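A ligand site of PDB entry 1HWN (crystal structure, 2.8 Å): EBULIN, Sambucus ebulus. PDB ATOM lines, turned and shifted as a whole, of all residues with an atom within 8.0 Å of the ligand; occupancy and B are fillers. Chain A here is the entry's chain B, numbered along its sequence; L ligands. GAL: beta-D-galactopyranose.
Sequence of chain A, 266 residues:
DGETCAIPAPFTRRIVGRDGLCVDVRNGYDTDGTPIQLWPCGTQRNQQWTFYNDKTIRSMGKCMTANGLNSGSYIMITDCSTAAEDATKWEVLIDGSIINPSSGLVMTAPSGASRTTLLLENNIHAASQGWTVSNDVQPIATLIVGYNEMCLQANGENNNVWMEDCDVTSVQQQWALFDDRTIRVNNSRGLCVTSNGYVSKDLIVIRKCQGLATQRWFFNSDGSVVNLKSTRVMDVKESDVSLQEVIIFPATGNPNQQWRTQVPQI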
ATOM      1  N   CYS A  22      26.402  22.302  -1.304  1.00  0.00           N
ATOM      2  CA  CYS A  22      27.731  21.800  -1.631  1.00  0.00           C
ATOM      3  C   CYS A  22      28.490  22.807  -2.495  1.00  0.00           C
ATOM      4  O   CYS A  22      27.900  23.498  -3.317  1.00  0.00           O
ATOM      5  CB  CYS A  22      27.631  20.473  -2.382  1.00  0.00           C
ATOM      6  SG  CYS A  22      26.865  19.132  -1.416  1.00  0.00           S
ATOM      7  N   VAL A  23      29.800  22.877  -2.279  1.00  0.00           N
ATOM      8  CA  VAL A  23      30.642  23.803  -3.038  1.00  0.00           C
ATOM      9  C   VAL A  23      30.705  23.341  -4.492  1.00  0.00           C
ATOM     10  O   VAL A  23      31.204  22.258  -4.800  1.00  0.00           O
ATOM     11  CB  VAL A  23      32.063  23.871  -2.438  1.00  0.00           C
ATOM     12  CG1 VAL A  23      32.782  22.536  -2.585  1.00  0.00           C
ATOM     13  CG2 VAL A  23      32.849  24.980  -3.100  1.00  0.00           C
ATOM     14  N   ASP A  24      30.170  24.169  -5.394  1.00  0.00           N
ATOM     15  CA  ASP A  24      30.141  23.841  -6.817  1.00  0.00           C
ATOM     16  C   ASP A  24      30.924  24.830  -7.672  1.00  0.00           C
ATOM     17  O   ASP A  24      31.093  25.997  -7.308  1.00  0.00           O
ATOM     18  CB  ASP A  24      28.685  23.776  -7.278  1.00  0.00           C
ATOM     19  CG  ASP A  24      28.511  24.172  -8.733  1.00  0.00           C
ATOM     20  OD1 ASP A  24      28.602  25.382  -9.040  1.00  0.00           O
ATOM     21  OD2 ASP A  24      28.295  23.272  -9.566  1.00  0.00           O
ATOM     22  N   VAL A  25      31.386  24.349  -8.821  1.00  0.00           N
ATOM     23  CA  VAL A  25      32.147  25.168  -9.757  1.00  0.00           C
ATOM     24  C   VAL A  25      31.184  25.925 -10.663  1.00  0.00           C
ATOM     25  O   VAL A  25      30.482  25.318 -11.485  1.00  0.00           O
ATOM     26  CB  VAL A  25      33.068  24.291 -10.635  1.00  0.00           C
ATOM     27  CG1 VAL A  25      33.881  25.169 -11.574  1.00  0.00           C
ATOM     28  CG2 VAL A  25      33.982  23.463  -9.748  1.00  0.00           C
ATOM     29  N   ARG A  26      31.142  27.242 -10.510  1.00  0.00           N
ATOM     30  CA  ARG A  26      30.252  28.097 -11.282  1.00  0.00           C
ATOM     31  C   ARG A  26      30.073  27.663 -12.731  1.00  0.00           C
ATOM     32  O   ARG A  26      31.035  27.509 -13.479  1.00  0.00           O
ATOM     33  CB  ARG A  26      30.746  29.546 -11.245  1.00  0.00           C
ATOM     34  CG  ARG A  26      29.650  30.567 -11.520  1.00  0.00           C
ATOM     35  CD  ARG A  26      29.973  31.909 -10.894  1.00  0.00           C
ATOM     36  NE  ARG A  26      31.042  32.596 -11.625  1.00  0.00           N
ATOM     37  CZ  ARG A  26      31.309  33.889 -11.522  1.00  0.00           C
ATOM     38  NH1 ARG A  26      30.586  34.656 -10.715  1.00  0.00           N
ATOM     39  NH2 ARG A  26      32.305  34.421 -12.217  1.00  0.00           N
ATOM     40  N   ASN A  27      28.804  27.487 -13.123  1.00  0.00           N
ATOM     41  CA  ASN A  27      28.441  27.082 -14.486  1.00  0.00           C
ATOM     42  C   ASN A  27      28.940  25.687 -14.883  1.00  0.00           C
ATOM     43  O   ASN A  27      28.402  25.086 -15.800  1.00  0.00           O
ATOM     44  CB  ASN A  27      28.964  28.114 -15.494  1.00  0.00           C
ATOM     45  CG  ASN A  27      28.126  29.375 -15.520  1.00  0.00           C
ATOM     46  OD1 ASN A  27      28.375  30.270 -16.323  1.00  0.00           O
ATOM     47  ND2 ASN A  27      27.138  29.460 -14.634  1.00  0.00           N
ATOM     48  N   GLY A  28      29.949  25.186 -14.177  1.00  0.00           N
ATOM     49  CA  GLY A  28      30.478  23.876 -14.485  1.00  0.00           C
ATOM     50  C   GLY A  28      31.617  23.931 -15.487  1.00  0.00           C
ATOM     51  O   GLY A  28      32.110  22.888 -15.923  1.00  0.00           O
ATOM     52  N   TYR A  29      32.048  25.144 -15.826  1.00  0.00           N
ATOM     53  CA  TYR A  29      33.146  25.325 -16.773  1.00  0.00           C
ATOM     54  C   TYR A  29      34.454  24.897 -16.130  1.00  0.00           C
ATOM     55  O   TYR A  29      34.760  25.292 -15.005  1.00  0.00           O
ATOM     56  CB  TYR A  29      33.235  26.793 -17.198  1.00  0.00           C
ATOM     57  CG  TYR A  29      32.087  27.284 -18.049  1.00  0.00           C
ATOM     58  CD1 TYR A  29      31.506  28.531 -17.816  1.00  0.00           C
ATOM     59  CD2 TYR A  29      31.583  26.506 -19.093  1.00  0.00           C
ATOM     60  CE1 TYR A  29      30.454  28.991 -18.603  1.00  0.00           C
ATOM     61  CE2 TYR A  29      30.539  26.959 -19.894  1.00  0.00           C
ATOM     62  CZ  TYR A  29      29.981  28.200 -19.645  1.00  0.00           C
ATOM     63  OH  TYR A  29      28.947  28.662 -20.431  1.00  0.00           O
ATOM     64  N   THR A  34      37.443  30.162 -13.350  1.00  0.00           N
ATOM     65  CA  THR A  34      36.049  30.040 -12.906  1.00  0.00           C
ATOM     66  C   THR A  34      35.972  29.987 -11.381  1.00  0.00           C
ATOM     67  O   THR A  34      36.495  29.068 -10.750  1.00  0.00           O
ATOM     68  CB  THR A  34      35.394  28.781 -13.491  1.00  0.00           C
ATOM     69  OG1 THR A  34      36.124  28.349 -14.641  1.00  0.00           O
ATOM     70  CG2 THR A  34      33.954  29.067 -13.883  1.00  0.00           C
ATOM     71  N   PRO A  35      35.302  30.989 -10.767  1.00  0.00           N
ATOM     72  CA  PRO A  35      35.149  31.039  -9.310  1.00  0.00           C
ATOM     73  C   PRO A  35      34.388  29.856  -8.725  1.00  0.00           C
ATOM     74  O   PRO A  35      33.741  29.103  -9.438  1.00  0.00           O
ATOM     75  CB  PRO A  35      34.414  32.364  -9.080  1.00  0.00           C
ATOM     76  CG  PRO A  35      34.574  33.144 -10.343  1.00  0.00           C
ATOM     77  CD  PRO A  35      34.647  32.124 -11.433  1.00  0.00           C
ATOM     78  N   ILE A  36      34.500  29.704  -7.406  1.00  0.00           N
ATOM     79  CA  ILE A  36      33.824  28.616  -6.694  1.00  0.00           C
ATOM     80  C   ILE A  36      32.783  29.217  -5.756  1.00  0.00           C
ATOM     81  O   ILE A  36      33.034  30.244  -5.118  1.00  0.00           O
ATOM     82  CB  ILE A  36      34.855  27.780  -5.876  1.00  0.00           C
ATOM     83  CG1 ILE A  36      35.020  26.399  -6.509  1.00  0.00           C
ATOM     84  CG2 ILE A  36      34.417  27.660  -4.413  1.00  0.00           C
ATOM     85  CD1 ILE A  36      33.839  25.480  -6.285  1.00  0.00           C
ATOM     86  N   GLN A  37      31.611  28.590  -5.691  1.00  0.00           N
ATOM     87  CA  GLN A  37      30.540  29.093  -4.835  1.00  0.00           C
ATOM     88  C   GLN A  37      29.609  27.982  -4.332  1.00  0.00           C
ATOM     89  O   GLN A  37      29.949  26.799  -4.383  1.00  0.00           O
ATOM     90  CB  GLN A  37      29.704  30.130  -5.593  1.00  0.00           C
ATOM     91  CG  GLN A  37      29.604  29.869  -7.092  1.00  0.00           C
ATOM     92  CD  GLN A  37      28.512  28.866  -7.422  1.00  0.00           C
ATOM     93  OE1 GLN A  37      27.373  29.250  -7.692  1.00  0.00           O
ATOM     94  NE2 GLN A  37      28.851  27.592  -7.404  1.00  0.00           N
ATOM     95  N   LEU A  38      28.442  28.381  -3.845  1.00  0.00           N
ATOM     96  CA  LEU A  38      27.456  27.437  -3.316  1.00  0.00           C
ATOM     97  C   LEU A  38      26.427  27.062  -4.380  1.00  0.00           C
ATOM     98  O   LEU A  38      26.174  27.830  -5.305  1.00  0.00           O
ATOM     99  CB  LEU A  38      26.737  28.055  -2.114  1.00  0.00           C
ATOM    100  CG  LEU A  38      27.091  27.535  -0.711  1.00  0.00           C
ATOM    101  CD1 LEU A  38      28.594  27.330  -0.583  1.00  0.00           C
ATOM    102  CD2 LEU A  38      26.600  28.531   0.327  1.00  0.00           C
ATOM    103  N   TRP A  39      25.856  25.876  -4.235  1.00  0.00           N
ATOM    104  CA  TRP A  39      24.854  25.385  -5.177  1.00  0.00           C
ATOM    105  C   TRP A  39      24.277  24.049  -4.722  1.00  0.00           C
ATOM    106  O   TRP A  39      25.016  23.162  -4.302  1.00  0.00           O
ATOM    107  CB  TRP A  39      25.463  25.220  -6.574  1.00  0.00           C
ATOM    108  CG  TRP A  39      24.444  25.039  -7.656  1.00  0.00           C
ATOM    109  CD1 TRP A  39      24.120  23.881  -8.287  1.00  0.00           C
ATOM    110  CD2 TRP A  39      23.621  26.057  -8.237  1.00  0.00           C
ATOM    111  NE1 TRP A  39      23.140  24.103  -9.228  1.00  0.00           N
ATOM    112  CE2 TRP A  39      22.822  25.436  -9.216  1.00  0.00           C
ATOM    113  CE3 TRP A  39      23.493  27.435  -8.026  1.00  0.00           C
ATOM    114  CZ2 TRP A  39      21.888  26.147  -9.978  1.00  0.00           C
ATOM    115  CZ3 TRP A  39      22.566  28.138  -8.788  1.00  0.00           C
ATOM    116  CH2 TRP A  39      21.774  27.497  -9.759  1.00  0.00           C
ATOM    117  N   PRO A  40      22.941  23.898  -4.792  1.00  0.00           N
ATOM    118  CA  PRO A  40      22.275  22.668  -4.385  1.00  0.00           C
ATOM    119  C   PRO A  40      23.025  21.411  -4.840  1.00  0.00           C
ATOM    120  O   PRO A  40      23.347  21.272  -6.016  1.00  0.00           O
ATOM    121  CB  PRO A  40      20.880  22.767  -5.037  1.00  0.00           C
ATOM    122  CG  PRO A  40      20.896  24.043  -5.846  1.00  0.00           C
ATOM    123  CD  PRO A  40      21.986  24.898  -5.290  1.00  0.00           C
ATOM    124  N   THR A  43      23.997  15.288  -8.781  1.00  0.00           N
ATOM    125  CA  THR A  43      24.898  14.529  -9.639  1.00  0.00           C
ATOM    126  C   THR A  43      25.520  15.432 -10.697  1.00  0.00           C
ATOM    127  O   THR A  43      24.874  15.743 -11.705  1.00  0.00           O
ATOM    128  CB  THR A  43      24.172  13.373 -10.348  1.00  0.00           C
ATOM    129  OG1 THR A  43      22.785  13.693 -10.487  1.00  0.00           O
ATOM    130  CG2 THR A  43      24.309  12.084  -9.550  1.00  0.00           C
ATOM    131  N   GLN A  44      26.762  15.855 -10.469  1.00  0.00           N
ATOM    132  CA  GLN A  44      27.460  16.725 -11.409  1.00  0.00           C
ATOM    133  C   GLN A  44      28.962  16.672 -11.173  1.00  0.00           C
ATOM    134  O   GLN A  44      29.419  16.521 -10.036  1.00  0.00           O
ATOM    135  CB  GLN A  44      26.970  18.167 -11.274  1.00  0.00           C
ATOM    136  CG  GLN A  44      26.206  18.443  -9.993  1.00  0.00           C
ATOM    137  CD  GLN A  44      25.315  19.653 -10.088  1.00  0.00           C
ATOM    138  OE1 GLN A  44      25.187  20.271 -11.147  1.00  0.00           O
ATOM    139  NE2 GLN A  44      24.677  20.005  -8.974  1.00  0.00           N
ATOM    140  N   ARG A  45      29.732  16.798 -12.251  1.00  0.00           N
ATOM    141  CA  ARG A  45      31.191  16.765 -12.174  1.00  0.00           C
ATOM    142  C   ARG A  45      31.753  18.027 -11.518  1.00  0.00           C
ATOM    143  O   ARG A  45      32.850  17.995 -10.943  1.00  0.00           O
ATOM    144  CB  ARG A  45      31.783  16.598 -13.572  1.00  0.00           C
ATOM    145  CG  ARG A  45      33.307  16.630 -13.604  1.00  0.00           C
ATOM    146  CD  ARG A  45      33.834  16.604 -15.033  1.00  0.00           C
ATOM    147  NE  ARG A  45      33.513  17.828 -15.767  1.00  0.00           N
ATOM    148  CZ  ARG A  45      33.656  17.978 -17.074  1.00  0.00           C
ATOM    149  NH1 ARG A  45      34.131  16.984 -17.809  1.00  0.00           N
ATOM    150  NH2 ARG A  45      33.332  19.127 -17.653  1.00  0.00           N
ATOM    151  N   ASN A  46      31.020  19.123 -11.616  1.00  0.00           N
ATOM    152  CA  ASN A  46      31.460  20.392 -11.047  1.00  0.00           C
ATOM    153  C   ASN A  46      31.203  20.459  -9.547  1.00  0.00           C
ATOM    154  O   ASN A  46      31.283  21.534  -8.949  1.00  0.00           O
ATOM    155  CB  ASN A  46      30.753  21.546 -11.745  1.00  0.00           C
ATOM    156  CG  ASN A  46      29.350  21.195 -12.184  1.00  0.00           C
ATOM    157  OD1 ASN A  46      29.150  20.347 -13.058  1.00  0.00           O
ATOM    158  ND2 ASN A  46      28.352  21.842 -11.583  1.00  0.00           N
ATOM    159  N   GLN A  47      30.884  19.319  -8.937  1.00  0.00           N
ATOM    160  CA  GLN A  47      30.620  19.283  -7.503  1.00  0.00           C
ATOM    161  C   GLN A  47      31.462  18.222  -6.801  1.00  0.00           C
ATOM    162  O   GLN A  47      31.641  18.271  -5.582  1.00  0.00           O
ATOM    163  CB  GLN A  47      29.134  19.029  -7.266  1.00  0.00           C
ATOM    164  CG  GLN A  47      28.222  20.029  -7.966  1.00  0.00           C
ATOM    165  CD  GLN A  47      27.161  20.611  -7.045  1.00  0.00           C
ATOM    166  OE1 GLN A  47      26.976  20.149  -5.921  1.00  0.00           O
ATOM    167  NE2 GLN A  47      26.463  21.638  -7.524  1.00  0.00           N
ATOM    168  N   SER A 114      21.990  30.598  -2.381  1.00  0.00           N
ATOM    169  CA  SER A 114      22.530  29.969  -3.582  1.00  0.00           C
ATOM    170  C   SER A 114      23.377  30.936  -4.397  1.00  0.00           C
ATOM    171  O   SER A 114      23.120  32.149  -4.403  1.00  0.00           O
ATOM    172  CB  SER A 114      21.393  29.430  -4.450  1.00  0.00           C
ATOM    173  OG  SER A 114      21.841  28.405  -5.321  1.00  0.00           O
ATOM    174  N   ARG A 115      24.386  30.401  -5.074  1.00  0.00           N
ATOM    175  CA  ARG A 115      25.289  31.190  -5.909  1.00  0.00           C
ATOM    176  C   ARG A 115      26.315  32.000  -5.124  1.00  0.00           C
ATOM    177  O   ARG A 115      27.261  32.534  -5.710  1.00  0.00           O
ATOM    178  CB  ARG A 115      24.487  32.129  -6.829  1.00  0.00           C
ATOM    179  CG  ARG A 115      24.639  31.837  -8.310  1.00  0.00           C
ATOM    180  CD  ARG A 115      23.287  31.784  -9.018  1.00  0.00           C
ATOM    181  NE  ARG A 115      23.367  31.106 -10.309  1.00  0.00           N
ATOM    182  CZ  ARG A 115      22.344  30.949 -11.136  1.00  0.00           C
ATOM    183  NH1 ARG A 115      21.145  31.444 -10.821  1.00  0.00           N
ATOM    184  NH2 ARG A 115      22.502  30.320 -12.294  1.00  0.00           N
ATOM    185  N   THR A 116      26.139  32.089  -3.810  1.00  0.00           N
ATOM    186  CA  THR A 116      27.075  32.835  -2.983  1.00  0.00           C
ATOM    187  C   THR A 116      28.512  32.391  -3.267  1.00  0.00           C
ATOM    188  O   THR A 116      28.917  31.288  -2.902  1.00  0.00           O
ATOM    189  CB  THR A 116      26.781  32.656  -1.482  1.00  0.00           C
ATOM    190  OG1 THR A 116      25.610  33.405  -1.141  1.00  0.00           O
ATOM    191  CG2 THR A 116      27.953  33.145  -0.634  1.00  0.00           C
HETATM  192  C1  GAL L   1      24.514  26.322 -13.487  1.00  0.00           C
HETATM  193  C2  GAL L   1      25.116  24.913 -13.607  1.00  0.00           C
HETATM  194  C3  GAL L   1      25.367  24.329 -12.219  1.00  0.00           C
HETATM  195  C4  GAL L   1      26.209  25.299 -11.376  1.00  0.00           C
HETATM  196  C5  GAL L   1      25.542  26.673 -11.353  1.00  0.00           C
HETATM  197  C6  GAL L   1      26.324  27.720 -10.598  1.00  0.00           C
HETATM  198  O1  GAL L   1      24.400  26.888 -14.752  1.00  0.00           O
HETATM  199  O2  GAL L   1      24.216  24.071 -14.319  1.00  0.00           O
HETATM  200  O3  GAL L   1      26.045  23.080 -12.339  1.00  0.00           O
HETATM  201  O4  GAL L   1      27.514  25.404 -11.940  1.00  0.00           O
HETATM  202  O5  GAL L   1      25.374  27.160 -12.707  1.00  0.00           O
HETATM  203  O6  GAL L   1      26.665  27.277  -9.288  1.00  0.00           O
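Arg 26 touches the ligand (C to O4, 3.5 Å). CE3 of Trp 39 touches O6 of the ligand, at 3.4 Å. Nine residues have an atom within 4 Å of the ligand: Asp 24, Val 25, Arg 26, Asn 27, Gly 28, Gln 37, Trp 39, Gln 44 and Asn 46. The nearest printed residue that does not touch the ligand is Leu 38 (4.1 Å).
The side-chain amide oxygen (OE1) of Gln 37 lies within hydrogen-bond range of an oxygen (O6) of the ligand, 2.6 Å away. O4 of the ligand lies within hydrogen-bond range of N of Asn 27, 2.7 Å away. The side-chain amide nitrogen (ND2) of Asn 27 lies within hydrogen-bond range of an oxygen (O5) of the ligand, at 3.5 Å. OD1 of Asp 24 sits at hydrogen-bond distance from O6 of the ligand, at 2.7 Å. An oxygen (O3) of the ligand is in hydrogen-bond range of the side-chain amide nitrogen (ND2) of Asn 46 (2.7 Å). O4 of the ligand sits at hydrogen-bond distance from O of Val 25 (3.0 Å). The side-chain amide oxygen (OE1) of Gln 44 is in hydrogen-bond range of an oxygen (O3) of the ligand (3.2 Å). An oxygen (O4) of the ligand sits at hydrogen-bond distance from the backbone NH (N) of Gly 28, 3.3 Å away.
The side-chain amide nitrogen (NE2) of Gln 37 lies within hydrogen-bond range of the backbone carbonyl oxygen (O) of Asp 24, at 2.8 Å. The side-chain amide nitrogen of Asn 46 sits at hydrogen-bond distance from the side-chain carboxylate of Asp 24 (2.5 Å). OD1 of Asp 24 lies within hydrogen-bond range of N of Arg 26, at 3.5 Å. The side-chain amide nitrogen (NE2) of Gln 47 lies close to the side-chain carboxylate (OD2) of Asp 24, 3.2 Å away. O of Asn 46 sits at hydrogen-bond distance from N of Val 25, 2.8 Å away. The side-chain amide nitrogen (NE2) of Gln 44 sits close to the side-chain amide nitrogen (NE2) of Gln 47 (2.8 Å). The side-chain amide nitrogen (NE2) of Gln 44 is in hydrogen-bond range of the backbone carbonyl oxygen (O) of Pro 40, at 3.5 Å. The backbone carbonyl oxygen (O) of Pro 35 is in hydrogen-bond range of the backbone NH (N) of Arg 26.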
